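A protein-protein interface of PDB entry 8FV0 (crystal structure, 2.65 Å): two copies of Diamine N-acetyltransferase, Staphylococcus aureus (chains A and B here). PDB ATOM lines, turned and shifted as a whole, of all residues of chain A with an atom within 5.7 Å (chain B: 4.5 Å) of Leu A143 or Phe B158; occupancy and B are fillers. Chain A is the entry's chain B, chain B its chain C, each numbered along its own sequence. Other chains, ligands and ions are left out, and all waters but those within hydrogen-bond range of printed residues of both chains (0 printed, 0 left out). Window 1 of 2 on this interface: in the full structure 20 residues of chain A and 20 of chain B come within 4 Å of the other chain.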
ATOM      1  N   TYR A 120      32.675 -18.805  19.288  1.00  0.00           N
ATOM      2  CA  TYR A 120      33.216 -19.116  20.604  1.00  0.00           C
ATOM      3  C   TYR A 120      34.244 -18.050  20.956  1.00  0.00           C
ATOM      4  O   TYR A 120      35.160 -17.789  20.167  1.00  0.00           O
ATOM      5  CB  TYR A 120      33.871 -20.499  20.624  1.00  0.00           C
ATOM      6  CG  TYR A 120      33.010 -21.613  20.070  1.00  0.00           C
ATOM      7  CD1 TYR A 120      32.950 -21.855  18.704  1.00  0.00           C
ATOM      8  CD2 TYR A 120      32.267 -22.431  20.912  1.00  0.00           C
ATOM      9  CE1 TYR A 120      32.166 -22.873  18.191  1.00  0.00           C
ATOM     10  CE2 TYR A 120      31.481 -23.453  20.408  1.00  0.00           C
ATOM     11  CZ  TYR A 120      31.435 -23.669  19.046  1.00  0.00           C
ATOM     12  OH  TYR A 120      30.657 -24.683  18.535  1.00  0.00           O
ATOM     13  N   GLY A 141      25.469 -19.408  25.574  1.00  0.00           N
ATOM     14  CA  GLY A 141      25.983 -20.448  26.446  1.00  0.00           C
ATOM     15  C   GLY A 141      27.322 -20.092  27.044  1.00  0.00           C
ATOM     16  O   GLY A 141      28.056 -19.253  26.520  1.00  0.00           O
ATOM     17  N   LEU A 142      27.638 -20.760  28.153  1.00  0.00           N
ATOM     18  CA  LEU A 142      28.933 -20.628  28.822  1.00  0.00           C
ATOM     19  C   LEU A 142      29.506 -22.033  28.988  1.00  0.00           C
ATOM     20  O   LEU A 142      29.168 -22.739  29.943  1.00  0.00           O
ATOM     21  CB  LEU A 142      28.797 -19.921  30.166  1.00  0.00           C
ATOM     22  CG  LEU A 142      30.047 -19.917  31.051  1.00  0.00           C
ATOM     23  CD1 LEU A 142      31.195 -19.167  30.389  1.00  0.00           C
ATOM     24  CD2 LEU A 142      29.740 -19.321  32.421  1.00  0.00           C
ATOM     25  N   LEU A 143      30.367 -22.438  28.056  1.00  0.00           N
ATOM     26  CA  LEU A 143      30.981 -23.759  28.074  1.00  0.00           C
ATOM     27  C   LEU A 143      32.243 -23.692  28.926  1.00  0.00           C
ATOM     28  O   LEU A 143      33.264 -23.144  28.495  1.00  0.00           O
ATOM     29  CB  LEU A 143      31.299 -24.214  26.653  1.00  0.00           C
ATOM     30  CG  LEU A 143      30.253 -23.847  25.598  1.00  0.00           C
ATOM     31  CD1 LEU A 143      30.636 -24.441  24.249  1.00  0.00           C
ATOM     32  CD2 LEU A 143      28.865 -24.303  26.024  1.00  0.00           C
ATOM     33  N   LYS A 144      32.173 -24.243  30.133  1.00  0.00           N
ATOM     34  CA  LYS A 144      33.282 -24.151  31.071  1.00  0.00           C
ATOM     35  C   LYS A 144      34.345 -25.190  30.739  1.00  0.00           C
ATOM     36  O   LYS A 144      34.033 -26.341  30.417  1.00  0.00           O
ATOM     37  CB  LYS A 144      32.784 -24.341  32.503  1.00  0.00           C
ATOM     38  CG  LYS A 144      31.723 -23.334  32.934  1.00  0.00           C
ATOM     39  CD  LYS A 144      31.224 -23.624  34.344  1.00  0.00           C
ATOM     40  CE  LYS A 144      29.971 -22.825  34.671  1.00  0.00           C
ATOM     41  NZ  LYS A 144      29.404 -23.188  36.002  1.00  0.00           N
ATOM     42  N   GLU A 145      35.607 -24.771  30.813  1.00  0.00           N
ATOM     43  CA  GLU A 145      36.737 -25.659  30.544  1.00  0.00           C
ATOM     44  C   GLU A 145      36.580 -26.351  29.192  1.00  0.00           C
ATOM     45  O   GLU A 145      36.908 -27.528  29.026  1.00  0.00           O
ATOM     46  CB  GLU A 145      36.901 -26.681  31.673  1.00  0.00           C
ATOM     47  CG  GLU A 145      37.195 -26.055  33.033  1.00  0.00           C
ATOM     48  CD  GLU A 145      37.369 -27.083  34.139  1.00  0.00           C
ATOM     49  OE1 GLU A 145      37.175 -28.287  33.874  1.00  0.00           O
ATOM     50  OE2 GLU A 145      37.701 -26.683  35.275  1.00  0.00           O
ATOM     51  N   GLN A 146      36.068 -25.604  28.210  1.00  0.00           N
ATOM     52  CA  GLN A 146      35.877 -26.141  26.869  1.00  0.00           C
ATOM     53  C   GLN A 146      37.172 -26.188  26.070  1.00  0.00           C
ATOM     54  O   GLN A 146      37.273 -26.977  25.124  1.00  0.00           O
ATOM     55  CB  GLN A 146      34.841 -25.301  26.115  1.00  0.00           C
ATOM     56  CG  GLN A 146      34.402 -25.891  24.785  1.00  0.00           C
ATOM     57  CD  GLN A 146      33.588 -27.156  24.953  1.00  0.00           C
ATOM     58  OE1 GLN A 146      32.995 -27.390  26.006  1.00  0.00           O
ATOM     59  NE2 GLN A 146      33.560 -27.984  23.916  1.00  0.00           N
ATOM     60  N   LYS A 154      39.981 -23.040  30.048  1.00  0.00           N
ATOM     61  CA  LYS A 154      39.352 -21.730  29.991  1.00  0.00           C
ATOM     62  C   LYS A 154      37.900 -21.859  29.559  1.00  0.00           C
ATOM     63  O   LYS A 154      37.569 -22.673  28.691  1.00  0.00           O
ATOM     64  CB  LYS A 154      40.117 -20.807  29.033  1.00  0.00           C
ATOM     65  CG  LYS A 154      41.607 -20.706  29.347  1.00  0.00           C
ATOM     66  CD  LYS A 154      42.218 -19.413  28.819  1.00  0.00           C
ATOM     67  CE  LYS A 154      41.778 -18.211  29.645  1.00  0.00           C
ATOM     68  NZ  LYS A 154      42.314 -16.930  29.106  1.00  0.00           N
ATOM     69  N   ASP A 155      37.036 -21.060  30.180  1.00  0.00           N
ATOM     70  CA  ASP A 155      35.629 -21.031  29.810  1.00  0.00           C
ATOM     71  C   ASP A 155      35.442 -20.208  28.542  1.00  0.00           C
ATOM     72  O   ASP A 155      36.183 -19.256  28.279  1.00  0.00           O
ATOM     73  CB  ASP A 155      34.785 -20.443  30.941  1.00  0.00           C
ATOM     74  CG  ASP A 155      34.954 -21.197  32.246  1.00  0.00           C
ATOM     75  OD1 ASP A 155      35.745 -22.163  32.280  1.00  0.00           O
ATOM     76  OD2 ASP A 155      34.295 -20.821  33.238  1.00  0.00           O
ATOM     77  N   ALA A 156      34.440 -20.583  27.752  1.00  0.00           N
ATOM     78  CA  ALA A 156      34.179 -19.935  26.476  1.00  0.00           C
ATOM     79  C   ALA A 156      32.700 -19.601  26.358  1.00  0.00           C
ATOM     80  O   ALA A 156      31.843 -20.460  26.583  1.00  0.00           O
ATOM     81  CB  ALA A 156      34.611 -20.826  25.305  1.00  0.00           C
ATOM     82  N   TYR A 157      32.410 -18.351  26.015  1.00  0.00           N
ATOM     83  CA  TYR A 157      31.056 -17.941  25.690  1.00  0.00           C
ATOM     84  C   TYR A 157      30.720 -18.374  24.270  1.00  0.00           C
ATOM     85  O   TYR A 157      31.458 -18.072  23.323  1.00  0.00           O
ATOM     86  CB  TYR A 157      30.913 -16.425  25.822  1.00  0.00           C
ATOM     87  CG  TYR A 157      30.773 -15.922  27.243  1.00  0.00           C
ATOM     88  CD1 TYR A 157      29.839 -16.472  28.109  1.00  0.00           C
ATOM     89  CD2 TYR A 157      31.572 -14.890  27.714  1.00  0.00           C
ATOM     90  CE1 TYR A 157      29.705 -16.010  29.404  1.00  0.00           C
ATOM     91  CE2 TYR A 157      31.450 -14.423  29.007  1.00  0.00           C
ATOM     92  CZ  TYR A 157      30.514 -14.987  29.848  1.00  0.00           C
ATOM     93  OH  TYR A 157      30.385 -14.525  31.138  1.00  0.00           O
ATOM     94  N   PHE A 158      29.625 -19.122  24.138  1.00  0.00           N
ATOM     95  CA  PHE A 158      29.004 -19.416  22.852  1.00  0.00           C
ATOM     96  C   PHE A 158      27.986 -18.312  22.588  1.00  0.00           C
ATOM     97  O   PHE A 158      26.936 -18.261  23.243  1.00  0.00           O
ATOM     98  CB  PHE A 158      28.337 -20.789  22.875  1.00  0.00           C
ATOM     99  CG  PHE A 158      27.746 -21.206  21.554  1.00  0.00           C
ATOM    100  CD1 PHE A 158      26.569 -20.637  21.091  1.00  0.00           C
ATOM    101  CD2 PHE A 158      28.358 -22.179  20.783  1.00  0.00           C
ATOM    102  CE1 PHE A 158      26.026 -21.021  19.879  1.00  0.00           C
ATOM    103  CE2 PHE A 158      27.817 -22.569  19.573  1.00  0.00           C
ATOM    104  CZ  PHE A 158      26.650 -21.990  19.122  1.00  0.00           C
ATOM    105  N   LYS B 116      36.253 -33.698  29.374  1.00  0.00           N
ATOM    106  CA  LYS B 116      34.889 -33.190  29.331  1.00  0.00           C
ATOM    107  C   LYS B 116      34.149 -33.878  28.197  1.00  0.00           C
ATOM    108  O   LYS B 116      34.743 -34.236  27.179  1.00  0.00           O
ATOM    109  CB  LYS B 116      34.874 -31.670  29.140  1.00  0.00           C
ATOM    110  CG  LYS B 116      33.489 -31.055  29.039  1.00  0.00           C
ATOM    111  CD  LYS B 116      33.582 -29.546  28.857  1.00  0.00           C
ATOM    112  CE  LYS B 116      32.207 -28.917  28.709  1.00  0.00           C
ATOM    113  NZ  LYS B 116      32.288 -27.437  28.558  1.00  0.00           N
ATOM    114  N   TYR B 118      30.333 -33.472  25.952  1.00  0.00           N
ATOM    115  CA  TYR B 118      29.242 -32.550  25.670  1.00  0.00           C
ATOM    116  C   TYR B 118      28.322 -33.151  24.615  1.00  0.00           C
ATOM    117  O   TYR B 118      28.667 -34.123  23.941  1.00  0.00           O
ATOM    118  CB  TYR B 118      29.763 -31.175  25.212  1.00  0.00           C
ATOM    119  CG  TYR B 118      30.596 -31.199  23.953  1.00  0.00           C
ATOM    120  CD1 TYR B 118      31.967 -31.418  24.008  1.00  0.00           C
ATOM    121  CD2 TYR B 118      30.017 -30.989  22.709  1.00  0.00           C
ATOM    122  CE1 TYR B 118      32.734 -31.436  22.859  1.00  0.00           C
ATOM    123  CE2 TYR B 118      30.776 -31.003  21.554  1.00  0.00           C
ATOM    124  CZ  TYR B 118      32.135 -31.228  21.636  1.00  0.00           C
ATOM    125  OH  TYR B 118      32.899 -31.246  20.492  1.00  0.00           O
ATOM    126  N   LEU B 119      27.135 -32.559  24.496  1.00  0.00           N
ATOM    127  CA  LEU B 119      26.106 -33.080  23.607  1.00  0.00           C
ATOM    128  C   LEU B 119      25.114 -31.975  23.284  1.00  0.00           C
ATOM    129  O   LEU B 119      24.948 -31.012  24.038  1.00  0.00           O
ATOM    130  CB  LEU B 119      25.385 -34.280  24.233  1.00  0.00           C
ATOM    131  CG  LEU B 119      24.563 -34.008  25.498  1.00  0.00           C
ATOM    132  CD1 LEU B 119      23.139 -33.566  25.165  1.00  0.00           C
ATOM    133  CD2 LEU B 119      24.549 -35.235  26.409  1.00  0.00           C
ATOM    134  N   TYR B 120      24.455 -32.132  22.135  1.00  0.00           N
ATOM    135  CA  TYR B 120      23.333 -31.297  21.725  1.00  0.00           C
ATOM    136  C   TYR B 120      22.064 -32.135  21.821  1.00  0.00           C
ATOM    137  O   TYR B 120      22.052 -33.291  21.385  1.00  0.00           O
ATOM    138  CB  TYR B 120      23.513 -30.785  20.293  1.00  0.00           C
ATOM    139  CG  TYR B 120      24.835 -30.102  20.033  1.00  0.00           C
ATOM    140  CD1 TYR B 120      25.974 -30.841  19.745  1.00  0.00           C
ATOM    141  CD2 TYR B 120      24.943 -28.718  20.064  1.00  0.00           C
ATOM    142  CE1 TYR B 120      27.186 -30.223  19.504  1.00  0.00           C
ATOM    143  CE2 TYR B 120      26.150 -28.090  19.824  1.00  0.00           C
ATOM    144  CZ  TYR B 120      27.268 -28.847  19.544  1.00  0.00           C
ATOM    145  OH  TYR B 120      28.473 -28.227  19.304  1.00  0.00           O
ATOM    146  N   LYS B 138      24.970 -31.373  32.725  1.00  0.00           N
ATOM    147  CA  LYS B 138      24.298 -30.130  33.076  1.00  0.00           C
ATOM    148  C   LYS B 138      24.218 -29.228  31.855  1.00  0.00           C
ATOM    149  O   LYS B 138      25.158 -29.157  31.057  1.00  0.00           O
ATOM    150  CB  LYS B 138      25.032 -29.422  34.219  1.00  0.00           C
ATOM    151  CG  LYS B 138      25.103 -30.252  35.496  1.00  0.00           C
ATOM    152  CD  LYS B 138      25.821 -29.519  36.620  1.00  0.00           C
ATOM    153  CE  LYS B 138      27.292 -29.311  36.303  1.00  0.00           C
ATOM    154  NZ  LYS B 138      28.040 -28.775  37.473  1.00  0.00           N
ATOM    155  N   THR B 139      23.083 -28.550  31.709  1.00  0.00           N
ATOM    156  CA  THR B 139      22.879 -27.644  30.587  1.00  0.00           C
ATOM    157  C   THR B 139      23.795 -26.435  30.728  1.00  0.00           C
ATOM    158  O   THR B 139      23.745 -25.723  31.738  1.00  0.00           O
ATOM    159  CB  THR B 139      21.417 -27.209  30.523  1.00  0.00           C
ATOM    160  OG1 THR B 139      20.586 -28.356  30.300  1.00  0.00           O
ATOM    161  CG2 THR B 139      21.197 -26.202  29.402  1.00  0.00           C
ATOM    162  N   GLU B 140      24.634 -26.209  29.717  1.00  0.00           N
ATOM    163  CA  GLU B 140      25.511 -25.050  29.684  1.00  0.00           C
ATOM    164  C   GLU B 140      25.119 -24.031  28.625  1.00  0.00           C
ATOM    165  O   GLU B 140      25.638 -22.910  28.651  1.00  0.00           O
ATOM    166  CB  GLU B 140      26.964 -25.483  29.439  1.00  0.00           C
ATOM    167  CG  GLU B 140      27.607 -26.184  30.621  1.00  0.00           C
ATOM    168  CD  GLU B 140      29.100 -26.379  30.441  1.00  0.00           C
ATOM    169  OE1 GLU B 140      29.543 -26.567  29.288  1.00  0.00           O
ATOM    170  OE2 GLU B 140      29.831 -26.338  31.452  1.00  0.00           O
ATOM    171  N   GLY B 141      24.239 -24.388  27.694  1.00  0.00           N
ATOM    172  CA  GLY B 141      23.814 -23.420  26.700  1.00  0.00           C
ATOM    173  C   GLY B 141      22.461 -23.746  26.122  1.00  0.00           C
ATOM    174  O   GLY B 141      22.022 -24.900  26.125  1.00  0.00           O
ATOM    175  N   ALA B 156      18.239 -25.975  20.843  1.00  0.00           N
ATOM    176  CA  ALA B 156      18.945 -27.147  21.340  1.00  0.00           C
ATOM    177  C   ALA B 156      19.702 -26.795  22.609  1.00  0.00           C
ATOM    178  O   ALA B 156      20.375 -25.764  22.670  1.00  0.00           O
ATOM    179  CB  ALA B 156      19.914 -27.691  20.281  1.00  0.00           C
ATOM    180  N   TYR B 157      19.580 -27.650  23.618  1.00  0.00           N
ATOM    181  CA  TYR B 157      20.410 -27.538  24.804  1.00  0.00           C
ATOM    182  C   TYR B 157      21.790 -28.110  24.503  1.00  0.00           C
ATOM    183  O   TYR B 157      21.914 -29.233  23.996  1.00  0.00           O
ATOM    184  CB  TYR B 157      19.783 -28.268  25.990  1.00  0.00           C
ATOM    185  CG  TYR B 157      18.563 -27.577  26.557  1.00  0.00           C
ATOM    186  CD1 TYR B 157      18.647 -26.297  27.087  1.00  0.00           C
ATOM    187  CD2 TYR B 157      17.329 -28.211  26.573  1.00  0.00           C
ATOM    188  CE1 TYR B 157      17.533 -25.663  27.608  1.00  0.00           C
ATOM    189  CE2 TYR B 157      16.211 -27.588  27.091  1.00  0.00           C
ATOM    190  CZ  TYR B 157      16.317 -26.314  27.607  1.00  0.00           C
ATOM    191  OH  TYR B 157      15.205 -25.692  28.123  1.00  0.00           O
ATOM    192  N   PHE B 158      22.815 -27.308  24.772  1.00  0.00           N
ATOM    193  CA  PHE B 158      24.200 -27.762  24.827  1.00  0.00           C
ATOM    194  C   PHE B 158      24.465 -28.166  26.272  1.00  0.00           C
ATOM    195  O   PHE B 158      24.556 -27.302  27.155  1.00  0.00           O
ATOM    196  CB  PHE B 158      25.147 -26.655  24.370  1.00  0.00           C
ATOM    197  CG  PHE B 158      26.585 -27.085  24.260  1.00  0.00           C
ATOM    198  CD1 PHE B 158      27.341 -27.328  25.396  1.00  0.00           C
ATOM    199  CD2 PHE B 158      27.187 -27.227  23.022  1.00  0.00           C
ATOM    200  CE1 PHE B 158      28.662 -27.719  25.297  1.00  0.00           C
ATOM    201  CE2 PHE B 158      28.510 -27.614  22.917  1.00  0.00           C
ATOM    202  CZ  PHE B 158      29.248 -27.859  24.057  1.00  0.00           C
ATOM    203  N   MET B 159      24.556 -29.473  26.514  1.00  0.00           N
ATOM    204  CA  MET B 159      24.770 -30.033  27.841  1.00  0.00           C
ATOM    205  C   MET B 159      26.149 -30.675  27.898  1.00  0.00           C
ATOM    206  O   MET B 159      26.744 -31.001  26.870  1.00  0.00           O
ATOM    207  CB  MET B 159      23.695 -31.072  28.177  1.00  0.00           C
ATOM    208  CG  MET B 159      22.289 -30.641  27.792  1.00  0.00           C
ATOM    209  SD  MET B 159      21.013 -31.807  28.308  1.00  0.00           S
ATOM    210  CE  MET B 159      21.156 -31.697  30.090  1.00  0.00           C
ATOM    211  N   SER B 160      26.659 -30.866  29.113  1.00  0.00           N
ATOM    212  CA  SER B 160      28.003 -31.409  29.236  1.00  0.00           C
ATOM    213  C   SER B 160      28.268 -31.889  30.653  1.00  0.00           C
ATOM    214  O   SER B 160      27.557 -31.543  31.597  1.00  0.00           O
ATOM    215  CB  SER B 160      29.053 -30.366  28.820  1.00  0.00           C
ATOM    216  OG  SER B 160      28.837 -29.135  29.492  1.00  0.00           O
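Of the printed residues of chain A, Phe B158 touches Leu A143 (3.4 Å). Of the printed residues of chain B, Leu A142 touches Glu B140 (3.0 Å). Of the printed residues of chain B, Gln A146 touches Lys B116 (2.6 Å) and Tyr B118 (3.7 Å). Printed residues of chain A within 4 Å of Gly B141: Gly A141 (3.7 Å). Of the printed residues of chain A, Tyr B118 touches Gln A146 (3.7 Å). The nearest printed residue of chain B that does not touch Lys A144 is Lys B138 (5.9 Å).
Gly A141 touches its own counterpart, Gly B141. 5 positions are printed for both chains. Of the 11 pairs that touch across the chains among the printed residues, 1 has its exchanged pair printed and touching as well.
NZ of Lys B116 lies within hydrogen-bond range of O of Lys A144 (2.8 Å). The side-chain amino group (NZ) of Lys B116 is in hydrogen-bond range of the side-chain amide oxygen (OE1) of Gln A146 (2.6 Å). The backbone carbonyl oxygen of Glu B140 is in hydrogen-bond range of the backbone NH of Leu A142 (3.0 Å). OE2 of Glu B140 sits at hydrogen-bond distance from N of Lys A144.
Among the printed residues, merely in contact across the chains: Gly A141 with Glu B140 (3.3 Å), Gly A141 with Gly B141 (3.7 Å), Leu A143 with Lys B116 (3.8 Å), Leu A143 with Glu B140 (3.4 Å), Leu A143 with Phe B158 (3.4 Å), Glu A145 with Lys B116 (3.9 Å) and Gln A146 with Tyr B118 (3.7 Å).
Printed residues of chain A that touch a printed residue of chain B: Gly A141, Leu A142, Leu A143, Lys A144, Glu A145 and Gln A146. Hydrophobic or aromatic side chains of chain A that line the printed part of chain B: Leu A143. Of the 13 printed residues of chain B, 5 touch a printed residue of chain A. Hydrophobic or aromatic side chains of chain B that line the printed part of chain A: Tyr B118 and Phe B158. Among the printed residues, 11 pairs touch across the chains. Among the printed residues, no Asp or Glu carboxylate lies within 4 Å of a Lys or Arg side-chain nitrogen of the other chain.
NZ of Lys B116 is in salt-bridge range of OE1 of Glu B140 (3.0 Å). The backbone NH (N) of Glu B140 is in hydrogen-bond range of the backbone carbonyl oxygen (O) of Phe B158, 2.8 Å away. The side-chain carboxylate of Glu B140 is in hydrogen-bond range of the side-chain hydroxyl of Ser B160 (2.7 Å). The backbone carbonyl oxygen (O) of Gly B141 lies within hydrogen-bond range of the backbone NH (N) of Phe B158 (2.9 Å). The backbone NH (N) of Leu A143 lies within hydrogen-bond range of the backbone carbonyl oxygen (O) of Ala A156 (2.9 Å). The side-chain carboxylate (OD1) of Asp A155 sits at hydrogen-bond distance from the backbone NH (N) of Glu A145 (3.0 Å).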
